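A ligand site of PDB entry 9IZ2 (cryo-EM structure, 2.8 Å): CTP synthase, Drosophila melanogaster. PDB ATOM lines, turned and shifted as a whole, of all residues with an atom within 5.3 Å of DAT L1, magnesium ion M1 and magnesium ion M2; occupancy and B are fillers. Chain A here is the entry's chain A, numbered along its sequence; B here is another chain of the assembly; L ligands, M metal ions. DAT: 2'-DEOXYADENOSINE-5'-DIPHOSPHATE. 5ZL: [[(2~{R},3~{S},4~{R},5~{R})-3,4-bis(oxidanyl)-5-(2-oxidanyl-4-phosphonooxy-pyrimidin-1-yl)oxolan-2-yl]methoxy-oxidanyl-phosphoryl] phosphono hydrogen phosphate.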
ATOM      1  N   SER A  12     -26.763  26.681  23.101  1.00  0.00           N
ATOM      2  CA  SER A  12     -27.265  25.342  23.386  1.00  0.00           C
ATOM      3  C   SER A  12     -26.161  24.309  23.501  1.00  0.00           C
ATOM      4  O   SER A  12     -26.454  23.133  23.741  1.00  0.00           O
ATOM      5  CB  SER A  12     -28.266  24.907  22.309  1.00  0.00           C
ATOM      6  OG  SER A  12     -27.609  24.538  21.114  1.00  0.00           O
ATOM      7  N   GLY A  13     -24.906  24.702  23.323  1.00  0.00           N
ATOM      8  CA  GLY A  13     -23.799  23.791  23.541  1.00  0.00           C
ATOM      9  C   GLY A  13     -23.112  24.074  24.853  1.00  0.00           C
ATOM     10  O   GLY A  13     -21.956  23.698  25.066  1.00  0.00           O
ATOM     11  N   VAL A  14     -23.831  24.766  25.747  1.00  0.00           N
ATOM     12  CA  VAL A  14     -23.215  25.267  26.972  1.00  0.00           C
ATOM     13  C   VAL A  14     -22.798  24.121  27.892  1.00  0.00           C
ATOM     14  O   VAL A  14     -21.770  24.200  28.564  1.00  0.00           O
ATOM     15  CB  VAL A  14     -24.181  26.254  27.676  1.00  0.00           C
ATOM     16  CG1 VAL A  14     -25.521  25.608  27.950  1.00  0.00           C
ATOM     17  CG2 VAL A  14     -23.552  26.785  28.950  1.00  0.00           C
ATOM     18  N   GLY A  15     -23.566  23.033  27.921  1.00  0.00           N
ATOM     19  CA  GLY A  15     -23.247  21.951  28.823  1.00  0.00           C
ATOM     20  C   GLY A  15     -24.386  21.475  29.700  1.00  0.00           C
ATOM     21  O   GLY A  15     -24.138  20.863  30.737  1.00  0.00           O
ATOM     22  N   LYS A  16     -25.623  21.740  29.296  1.00  0.00           N
ATOM     23  CA  LYS A  16     -26.774  21.292  30.075  1.00  0.00           C
ATOM     24  C   LYS A  16     -26.796  19.777  30.229  1.00  0.00           C
ATOM     25  O   LYS A  16     -27.175  19.269  31.290  1.00  0.00           O
ATOM     26  CB  LYS A  16     -28.076  21.743  29.414  1.00  0.00           C
ATOM     27  CG  LYS A  16     -28.275  23.226  29.334  1.00  0.00           C
ATOM     28  CD  LYS A  16     -29.594  23.513  28.660  1.00  0.00           C
ATOM     29  CE  LYS A  16     -29.650  22.905  27.273  1.00  0.00           C
ATOM     30  NZ  LYS A  16     -28.672  23.529  26.350  1.00  0.00           N
ATOM     31  N   GLY A  17     -26.415  19.051  29.183  1.00  0.00           N
ATOM     32  CA  GLY A  17     -26.426  17.596  29.278  1.00  0.00           C
ATOM     33  C   GLY A  17     -25.464  17.069  30.321  1.00  0.00           C
ATOM     34  O   GLY A  17     -25.805  16.168  31.093  1.00  0.00           O
ATOM     35  N   VAL A  18     -24.256  17.628  30.355  1.00  0.00           N
ATOM     36  CA  VAL A  18     -23.260  17.202  31.337  1.00  0.00           C
ATOM     37  C   VAL A  18     -23.684  17.622  32.745  1.00  0.00           C
ATOM     38  O   VAL A  18     -23.504  16.874  33.703  1.00  0.00           O
ATOM     39  CB  VAL A  18     -21.874  17.754  30.964  1.00  0.00           C
ATOM     40  CG1 VAL A  18     -20.892  17.558  32.101  1.00  0.00           C
ATOM     41  CG2 VAL A  18     -21.372  17.083  29.704  1.00  0.00           C
ATOM     42  N   LYS A  38     -35.302  14.099  28.534  1.00  0.00           N
ATOM     43  CA  LYS A  38     -34.782  15.118  27.638  1.00  0.00           C
ATOM     44  C   LYS A  38     -35.941  15.707  26.861  1.00  0.00           C
ATOM     45  O   LYS A  38     -36.741  14.974  26.271  1.00  0.00           O
ATOM     46  CB  LYS A  38     -33.735  14.531  26.687  1.00  0.00           C
ATOM     47  CG  LYS A  38     -33.215  15.520  25.666  1.00  0.00           C
ATOM     48  CD  LYS A  38     -32.561  16.710  26.326  1.00  0.00           C
ATOM     49  CE  LYS A  38     -32.337  17.822  25.328  1.00  0.00           C
ATOM     50  NZ  LYS A  38     -31.501  17.365  24.187  1.00  0.00           N
ATOM     51  N   HIS A  55     -26.804  18.377  15.762  1.00  0.00           N
ATOM     52  CA  HIS A  55     -26.681  18.395  17.211  1.00  0.00           C
ATOM     53  C   HIS A  55     -25.671  17.398  17.761  1.00  0.00           C
ATOM     54  O   HIS A  55     -25.542  17.293  18.984  1.00  0.00           O
ATOM     55  CB  HIS A  55     -28.052  18.129  17.867  1.00  0.00           C
ATOM     56  CG  HIS A  55     -29.153  18.985  17.334  1.00  0.00           C
ATOM     57  ND1 HIS A  55     -29.402  20.260  17.796  1.00  0.00           N
ATOM     58  CD2 HIS A  55     -30.086  18.747  16.378  1.00  0.00           C
ATOM     59  CE1 HIS A  55     -30.424  20.770  17.154  1.00  0.00           C
ATOM     60  NE2 HIS A  55     -30.867  19.879  16.292  1.00  0.00           N
ATOM     61  N   ASP A  68     -31.238  11.848  20.970  1.00  0.00           N
ATOM     62  CA  ASP A  68     -30.108  12.757  21.103  1.00  0.00           C
ATOM     63  C   ASP A  68     -28.959  12.073  21.845  1.00  0.00           C
ATOM     64  O   ASP A  68     -29.131  11.038  22.492  1.00  0.00           O
ATOM     65  CB  ASP A  68     -30.532  14.014  21.861  1.00  0.00           C
ATOM     66  CG  ASP A  68     -30.165  15.285  21.125  1.00  0.00           C
ATOM     67  OD1 ASP A  68     -30.729  15.535  20.043  1.00  0.00           O
ATOM     68  OD2 ASP A  68     -29.324  16.042  21.639  1.00  0.00           O
ATOM     69  N   LEU A  69     -27.773  12.673  21.742  1.00  0.00           N
ATOM     70  CA  LEU A  69     -26.637  12.189  22.513  1.00  0.00           C
ATOM     71  C   LEU A  69     -26.769  12.471  24.000  1.00  0.00           C
ATOM     72  O   LEU A  69     -25.994  11.922  24.791  1.00  0.00           O
ATOM     73  CB  LEU A  69     -25.338  12.784  21.968  1.00  0.00           C
ATOM     74  CG  LEU A  69     -25.079  14.302  21.980  1.00  0.00           C
ATOM     75  CD1 LEU A  69     -24.548  14.801  23.313  1.00  0.00           C
ATOM     76  CD2 LEU A  69     -24.120  14.666  20.864  1.00  0.00           C
ATOM     77  N   ASP A  70     -27.722  13.317  24.391  1.00  0.00           N
ATOM     78  CA  ASP A  70     -27.983  13.537  25.810  1.00  0.00           C
ATOM     79  C   ASP A  70     -28.452  12.256  26.492  1.00  0.00           C
ATOM     80  O   ASP A  70     -28.060  11.968  27.626  1.00  0.00           O
ATOM     81  CB  ASP A  70     -29.002  14.658  25.998  1.00  0.00           C
ATOM     82  CG  ASP A  70     -28.453  16.010  25.609  1.00  0.00           C
ATOM     83  OD1 ASP A  70     -27.237  16.234  25.748  1.00  0.00           O
ATOM     84  OD2 ASP A  70     -29.249  16.874  25.181  1.00  0.00           O
ATOM     85  N   ASN A  73     -25.450  10.177  27.083  1.00  0.00           N
ATOM     86  CA  ASN A  73     -24.769  10.621  28.284  1.00  0.00           C
ATOM     87  C   ASN A  73     -25.484  10.148  29.547  1.00  0.00           C
ATOM     88  O   ASN A  73     -24.840   9.738  30.522  1.00  0.00           O
ATOM     89  CB  ASN A  73     -24.644  12.149  28.295  1.00  0.00           C
ATOM     90  CG  ASN A  73     -23.611  12.653  27.317  1.00  0.00           C
ATOM     91  OD1 ASN A  73     -22.670  11.936  26.955  1.00  0.00           O
ATOM     92  ND2 ASN A  73     -23.767  13.893  26.877  1.00  0.00           N
ATOM     93  N   TYR A  74     -26.817  10.202  29.538  1.00  0.00           N
ATOM     94  CA  TYR A  74     -27.583   9.732  30.689  1.00  0.00           C
ATOM     95  C   TYR A  74     -27.321   8.263  30.956  1.00  0.00           C
ATOM     96  O   TYR A  74     -27.077   7.859  32.094  1.00  0.00           O
ATOM     97  CB  TYR A  74     -29.083   9.964  30.481  1.00  0.00           C
ATOM     98  CG  TYR A  74     -29.506  11.386  30.206  1.00  0.00           C
ATOM     99  CD1 TYR A  74     -28.731  12.457  30.625  1.00  0.00           C
ATOM    100  CD2 TYR A  74     -30.696  11.646  29.547  1.00  0.00           C
ATOM    101  CE1 TYR A  74     -29.125  13.755  30.369  1.00  0.00           C
ATOM    102  CE2 TYR A  74     -31.100  12.946  29.292  1.00  0.00           C
ATOM    103  CZ  TYR A  74     -30.311  13.995  29.701  1.00  0.00           C
ATOM    104  OH  TYR A  74     -30.708  15.279  29.449  1.00  0.00           O
ATOM    105  N   GLU A 145     -34.348  18.083  31.272  1.00  0.00           N
ATOM    106  CA  GLU A 145     -33.457  19.015  30.584  1.00  0.00           C
ATOM    107  C   GLU A 145     -34.225  19.638  29.429  1.00  0.00           C
ATOM    108  O   GLU A 145     -34.788  18.935  28.597  1.00  0.00           O
ATOM    109  CB  GLU A 145     -32.206  18.300  30.080  1.00  0.00           C
ATOM    110  CG  GLU A 145     -31.281  19.206  29.281  1.00  0.00           C
ATOM    111  CD  GLU A 145     -30.200  18.442  28.568  1.00  0.00           C
ATOM    112  OE1 GLU A 145     -29.928  17.289  28.967  1.00  0.00           O
ATOM    113  OE2 GLU A 145     -29.624  18.988  27.601  1.00  0.00           O
ATOM    114  N   ARG A 216     -20.761  28.966  33.041  1.00  0.00           N
ATOM    115  CA  ARG A 216     -19.818  28.180  32.256  1.00  0.00           C
ATOM    116  C   ARG A 216     -18.825  29.106  31.558  1.00  0.00           C
ATOM    117  O   ARG A 216     -19.224  30.056  30.878  1.00  0.00           O
ATOM    118  CB  ARG A 216     -20.556  27.332  31.224  1.00  0.00           C
ATOM    119  CG  ARG A 216     -21.342  26.177  31.820  1.00  0.00           C
ATOM    120  CD  ARG A 216     -20.447  24.994  32.164  1.00  0.00           C
ATOM    121  NE  ARG A 216     -19.788  24.443  30.981  1.00  0.00           N
ATOM    122  CZ  ARG A 216     -18.530  24.683  30.640  1.00  0.00           C
ATOM    123  NH1 ARG A 216     -17.742  25.432  31.393  1.00  0.00           N
ATOM    124  NH2 ARG A 216     -18.049  24.146  29.522  1.00  0.00           N
ATOM    125  N   ILE A 243     -18.381  26.507  36.679  1.00  0.00           N
ATOM    126  CA  ILE A 243     -17.866  25.298  36.070  1.00  0.00           C
ATOM    127  C   ILE A 243     -17.097  25.700  34.819  1.00  0.00           C
ATOM    128  O   ILE A 243     -17.694  26.231  33.873  1.00  0.00           O
ATOM    129  CB  ILE A 243     -18.988  24.303  35.729  1.00  0.00           C
ATOM    130  CG1 ILE A 243     -19.855  24.007  36.949  1.00  0.00           C
ATOM    131  CG2 ILE A 243     -18.408  23.015  35.164  1.00  0.00           C
ATOM    132  CD1 ILE A 243     -19.142  23.222  38.023  1.00  0.00           C
ATOM    133  N   HIS A 244     -15.799  25.456  34.813  1.00  0.00           N
ATOM    134  CA  HIS A 244     -14.960  25.775  33.681  1.00  0.00           C
ATOM    135  C   HIS A 244     -14.657  24.510  32.881  1.00  0.00           C
ATOM    136  O   HIS A 244     -15.043  23.400  33.260  1.00  0.00           O
ATOM    137  CB  HIS A 244     -13.672  26.469  34.139  1.00  0.00           C
ATOM    138  CG  HIS A 244     -12.851  25.664  35.086  1.00  0.00           C
ATOM    139  ND1 HIS A 244     -13.020  25.716  36.450  1.00  0.00           N
ATOM    140  CD2 HIS A 244     -11.843  24.773  34.865  1.00  0.00           C
ATOM    141  CE1 HIS A 244     -12.152  24.905  37.028  1.00  0.00           C
ATOM    142  NE2 HIS A 244     -11.429  24.317  36.085  1.00  0.00           N
ATOM    143  N   ASP A 245     -13.974  24.679  31.758  1.00  0.00           N
ATOM    144  CA  ASP A 245     -13.616  23.550  30.904  1.00  0.00           C
ATOM    145  C   ASP A 245     -12.597  22.675  31.625  1.00  0.00           C
ATOM    146  O   ASP A 245     -11.487  23.128  31.937  1.00  0.00           O
ATOM    147  CB  ASP A 245     -13.082  24.036  29.573  1.00  0.00           C
ATOM    148  CG  ASP A 245     -14.163  24.609  28.680  1.00  0.00           C
ATOM    149  OD1 ASP A 245     -15.308  24.754  29.157  1.00  0.00           O
ATOM    150  OD2 ASP A 245     -13.869  24.929  27.514  1.00  0.00           O
ATOM    151  N   LEU A 246     -12.970  21.429  31.895  1.00  0.00           N
ATOM    152  CA  LEU A 246     -12.127  20.487  32.610  1.00  0.00           C
ATOM    153  C   LEU A 246     -11.500  19.498  31.646  1.00  0.00           C
ATOM    154  O   LEU A 246     -11.879  19.401  30.482  1.00  0.00           O
ATOM    155  CB  LEU A 246     -12.960  19.774  33.685  1.00  0.00           C
ATOM    156  CG  LEU A 246     -13.603  20.681  34.730  1.00  0.00           C
ATOM    157  CD1 LEU A 246     -14.780  19.997  35.393  1.00  0.00           C
ATOM    158  CD2 LEU A 246     -12.588  21.106  35.769  1.00  0.00           C
ATOM    159  N   ILE A 249     -14.977  14.892  31.588  1.00  0.00           N
ATOM    160  CA  ILE A 249     -16.288  15.106  32.202  1.00  0.00           C
ATOM    161  C   ILE A 249     -16.463  14.321  33.494  1.00  0.00           C
ATOM    162  O   ILE A 249     -17.529  14.405  34.111  1.00  0.00           O
ATOM    163  CB  ILE A 249     -17.431  14.755  31.238  1.00  0.00           C
ATOM    164  CG1 ILE A 249     -17.297  13.308  30.754  1.00  0.00           C
ATOM    165  CG2 ILE A 249     -17.435  15.718  30.059  1.00  0.00           C
ATOM    166  CD1 ILE A 249     -18.396  12.881  29.821  1.00  0.00           C
ATOM    167  N   VAL A 252     -16.510  16.971  36.421  1.00  0.00           N
ATOM    168  CA  VAL A 252     -17.676  17.823  36.639  1.00  0.00           C
ATOM    169  C   VAL A 252     -18.449  17.441  37.899  1.00  0.00           C
ATOM    170  O   VAL A 252     -18.770  18.353  38.694  1.00  0.00           O
ATOM    171  CB  VAL A 252     -18.559  17.858  35.383  1.00  0.00           C
ATOM    172  CG1 VAL A 252     -19.661  18.887  35.534  1.00  0.00           C
ATOM    173  CG2 VAL A 252     -17.717  18.147  34.147  1.00  0.00           C
ATOM    174  N   ASP A 312     -18.124  16.315  17.775  1.00  0.00           N
ATOM    175  CA  ASP A 312     -19.160  15.621  18.528  1.00  0.00           C
ATOM    176  C   ASP A 312     -20.029  14.739  17.651  1.00  0.00           C
ATOM    177  O   ASP A 312     -20.981  14.131  18.150  1.00  0.00           O
ATOM    178  CB  ASP A 312     -20.034  16.624  19.276  1.00  0.00           C
ATOM    179  CG  ASP A 312     -19.392  17.128  20.549  1.00  0.00           C
ATOM    180  OD1 ASP A 312     -18.730  16.330  21.236  1.00  0.00           O
ATOM    181  OD2 ASP A 312     -19.531  18.327  20.857  1.00  0.00           O
ATOM    182  N   ALA B 187     -14.896  23.532  23.801  1.00  0.00           N
ATOM    183  CA  ALA B 187     -15.837  22.502  24.251  1.00  0.00           C
ATOM    184  C   ALA B 187     -16.913  22.271  23.192  1.00  0.00           C
ATOM    185  O   ALA B 187     -17.093  21.145  22.717  1.00  0.00           O
ATOM    186  CB  ALA B 187     -16.466  22.894  25.570  1.00  0.00           C
ATOM    187  N   THR B 188     -17.626  23.331  22.830  1.00  0.00           N
ATOM    188  CA  THR B 188     -18.635  23.225  21.778  1.00  0.00           C
ATOM    189  C   THR B 188     -17.996  23.025  20.419  1.00  0.00           C
ATOM    190  O   THR B 188     -18.536  22.296  19.575  1.00  0.00           O
ATOM    191  CB  THR B 188     -19.516  24.481  21.792  1.00  0.00           C
ATOM    192  OG1 THR B 188     -19.964  24.737  23.120  1.00  0.00           O
ATOM    193  CG2 THR B 188     -20.724  24.285  20.889  1.00  0.00           C
HETATM  194  PB  DAT L   1     -25.952  20.822  25.979  1.00  0.00           P
HETATM  195  O1B DAT L   1     -26.184  22.245  26.392  1.00  0.00           O
HETATM  196  O2B DAT L   1     -25.818  20.618  24.497  1.00  0.00           O
HETATM  197  O3B DAT L   1     -26.856  19.818  26.633  1.00  0.00           O
HETATM  198  PA  DAT L   1     -23.713  19.108  26.347  1.00  0.00           P
HETATM  199  O1A DAT L   1     -22.867  18.887  27.556  1.00  0.00           O
HETATM  200  O2A DAT L   1     -24.687  18.042  25.911  1.00  0.00           O
HETATM  201  O3A DAT L   1     -24.497  20.498  26.542  1.00  0.00           O
HETATM  202  O5' DAT L   1     -22.730  19.445  25.130  1.00  0.00           O
HETATM  203  C5' DAT L   1     -21.609  20.302  25.326  1.00  0.00           C
HETATM  204  C4' DAT L   1     -20.315  19.574  24.985  1.00  0.00           C
HETATM  205  O4' DAT L   1     -19.222  20.165  25.686  1.00  0.00           O
HETATM  206  C3' DAT L   1     -20.382  18.113  25.386  1.00  0.00           C
HETATM  207  O3' DAT L   1     -20.066  17.288  24.278  1.00  0.00           O
HETATM  208  C2' DAT L   1     -19.377  17.929  26.508  1.00  0.00           C
HETATM  209  C1' DAT L   1     -18.626  19.238  26.608  1.00  0.00           C
HETATM  210  N9  DAT L   1     -18.712  19.792  27.985  1.00  0.00           N
HETATM  211  C8  DAT L   1     -19.834  19.982  28.684  1.00  0.00           C
HETATM  212  N7  DAT L   1     -19.566  20.507  29.907  1.00  0.00           N
HETATM  213  C5  DAT L   1     -18.239  20.662  29.994  1.00  0.00           C
HETATM  214  C6  DAT L   1     -17.287  21.169  31.004  1.00  0.00           C
HETATM  215  N6  DAT L   1     -17.711  21.622  32.206  1.00  0.00           N
HETATM  216  N1  DAT L   1     -15.974  21.156  30.688  1.00  0.00           N
HETATM  217  C2  DAT L   1     -15.534  20.714  29.503  1.00  0.00           C
HETATM  218  N3  DAT L   1     -16.337  20.239  28.538  1.00  0.00           N
HETATM  219  C4  DAT L   1     -17.682  20.189  28.722  1.00  0.00           C
HETATM  220  C21 5ZL L   2     -34.100  24.955  18.288  1.00  0.00           C
HETATM  221  C22 5ZL L   2     -33.826  24.276  19.584  1.00  0.00           C
HETATM  222  C24 5ZL L   2     -33.565  22.788  19.119  1.00  0.00           C
HETATM  223  C26 5ZL L   2     -33.280  21.052  20.747  1.00  0.00           C
HETATM  224  C28 5ZL L   2     -30.763  21.783  21.289  1.00  0.00           C
HETATM  225  C23 5ZL L   2     -33.339  24.306  17.373  1.00  0.00           C
HETATM  226  C25 5ZL L   2     -32.107  25.103  17.056  1.00  0.00           C
HETATM  227  C27 5ZL L   2     -31.526  22.456  20.358  1.00  0.00           C
HETATM  228  C29 5ZL L   2     -31.362  20.721  21.927  1.00  0.00           C
HETATM  229  N19 5ZL L   2     -32.755  22.075  20.121  1.00  0.00           N
HETATM  230  N20 5ZL L   2     -32.604  20.380  21.641  1.00  0.00           N
HETATM  231  O04 5ZL L   2     -32.921  22.893  18.008  1.00  0.00           O
HETATM  232  O05 5ZL L   2     -35.537  24.795  17.937  1.00  0.00           O
HETATM  233  O07 5ZL L   2     -31.004  24.544  17.811  1.00  0.00           O
HETATM  234  O08 5ZL L   2     -34.592  20.689  20.459  1.00  0.00           O
HETATM  235  O09 5ZL L   2     -29.819  26.903  17.338  1.00  0.00           O
HETATM  236  O10 5ZL L   2     -29.760  25.845  19.608  1.00  0.00           O
HETATM  237  O11 5ZL L   2     -28.438  24.805  17.860  1.00  0.00           O
HETATM  238  O12 5ZL L   2     -30.669  19.971  22.895  1.00  0.00           O
HETATM  239  O13 5ZL L   2     -27.735  28.440  16.393  1.00  0.00           O
HETATM  240  O14 5ZL L   2     -29.842  27.908  14.966  1.00  0.00           O
HETATM  241  O15 5ZL L   2     -28.280  26.100  15.414  1.00  0.00           O
HETATM  242  O16 5ZL L   2     -25.234  28.290  15.906  1.00  0.00           O
HETATM  243  O17 5ZL L   2     -26.196  26.635  17.365  1.00  0.00           O
HETATM  244  O18 5ZL L   2     -25.919  28.907  18.144  1.00  0.00           O
HETATM  245  O31 5ZL L   2     -29.838  21.989  24.231  1.00  0.00           O
HETATM  246  O32 5ZL L   2     -28.247  20.805  22.781  1.00  0.00           O
HETATM  247  O33 5ZL L   2     -29.057  19.720  24.889  1.00  0.00           O
HETATM  248  P01 5ZL L   2     -29.728  25.523  18.174  1.00  0.00           P
HETATM  249  P02 5ZL L   2     -28.925  27.301  15.990  1.00  0.00           P
HETATM  250  P03 5ZL L   2     -26.233  28.061  16.964  1.00  0.00           P
HETATM  251  P30 5ZL L   2     -29.437  20.642  23.718  1.00  0.00           P
HETATM  252 MG    MG M   1     -28.162  18.286  26.090  1.00  0.00          MG
HETATM  253 MG    MG M   2     -26.630  19.570  22.419  1.00  0.00          MG
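An oxygen (O3A) of DAT L1 sits close to the backbone NH (N) of Gly 15 (3.0 Å). The backbone carbonyl oxygen (O) of His 244 is in hydrogen-bond range of a nitrogen (N6) of DAT L1 (3.4 Å). An oxygen (O3') of DAT L1 is in hydrogen-bond range of the side-chain carboxylate (OD1) of Asp 312 (3.5 Å). NZ of Lys 16 is in salt-bridge range of O31 of 5ZL L2 (2.9 Å). N of Leu 246 is in hydrogen-bond range of N1 of DAT L1, 3.2 Å away. NZ of Lys 16 is in salt-bridge range of O1B of DAT L1, at 2.8 Å. N of Lys 16 sits at hydrogen-bond distance from O1B of DAT L1 (3.0 Å). O2B of DAT L1 lies close to O of Ser 12. The side-chain hydroxyl (OG) of Ser 12 sits at hydrogen-bond distance from an oxygen (O10) of 5ZL L2. O12 of 5ZL L2 lies within hydrogen-bond range of NZ of Lys 38 (3.0 Å). The backbone NH of Gly 17 sits close to an oxygen (O3B) of DAT L1 (2.7 Å). N of Val 18 lies close to O1A of DAT L1 (3.4 Å).
Merely in contact with magnesium ion M1: Gly 17 and Lys 38. Four residues have an atom within 4 Å of magnesium ion M1: Gly 17, Lys 38, Asp 70 and Glu 145.
Residues that only touch magnesium ion M2: Ser 12 (3.8 Å). Of the 25 residues printed, 1 comes within 4 Å of magnesium ion M2. The nearest printed residue that does not touch magnesium ion M2 is His 55 (4.3 Å).
Magnesium ion M1 is bound by OD2 of Asp 70, at 2.0 Å. Magnesium ion M1 is bound by O33 of 5ZL L2, at 2.1 Å. O3B of DAT L1 binds magnesium ion M1, 2.1 Å away. OE2 of Glu 145 binds magnesium ion M1 (2.2 Å). Magnesium ion M1 is bound by the side-chain carboxylate (OD1) of Asp 70.
Gly 13 touches DAT L1 (O to C5', 3.4 Å). N of Val 14 touches O1B of DAT L1 (3.5 Å). Arg 216 touches DAT L1 (NH2 to C6, 3.4 Å). CG2 of Ile 243 touches N6 of DAT L1, 3.3 Å away. CA of Asp 245 touches N1 of DAT L1, at 3.4 Å. Val 252 touches DAT L1 (CG2 to N6, 3.98 Å). Ala 187 of chain B touches DAT L1 (O to O4', 3.8 Å). Of the 25 residues printed, 17 come within 4 Å of DAT L1. Along chain A the residues within 4 Å of DAT L1 span positions 12 to 312. The nearest printed residue that does not touch DAT L1 is Leu 69 (4.2 Å).
NH2 of Arg 216 is in salt-bridge range of OD1 of Asp 245, 2.8 Å away. O of Ile 243 sits at hydrogen-bond distance from NH1 of Arg 216, 2.6 Å away. The side-chain amino group (NZ) of Lys 38 is in salt-bridge range of the side-chain carboxylate (OD2) of Asp 68. The backbone carbonyl oxygen (O) of Val 14 is in hydrogen-bond range of the guanidinium group (NE) of Arg 216 (3.1 Å). The side-chain amino group (NZ) of Lys 16 is in hydrogen-bond range of the backbone carbonyl oxygen (O) of Ser 12, at 3.4 Å. OD2 of Asp 70 sits close to NZ of Lys 38 (2.5 Å). O of Gly 13 is in hydrogen-bond range of OG1 of Thr 188 of chain B, at 3.0 Å.
Magnesium ion M2 is bound by an oxygen (O32) of 5ZL L2 (2.1 Å) and an oxygen (O2B) of DAT L1 (2.5 Å). Magnesium ion M2 has two donor atoms within binding distance.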
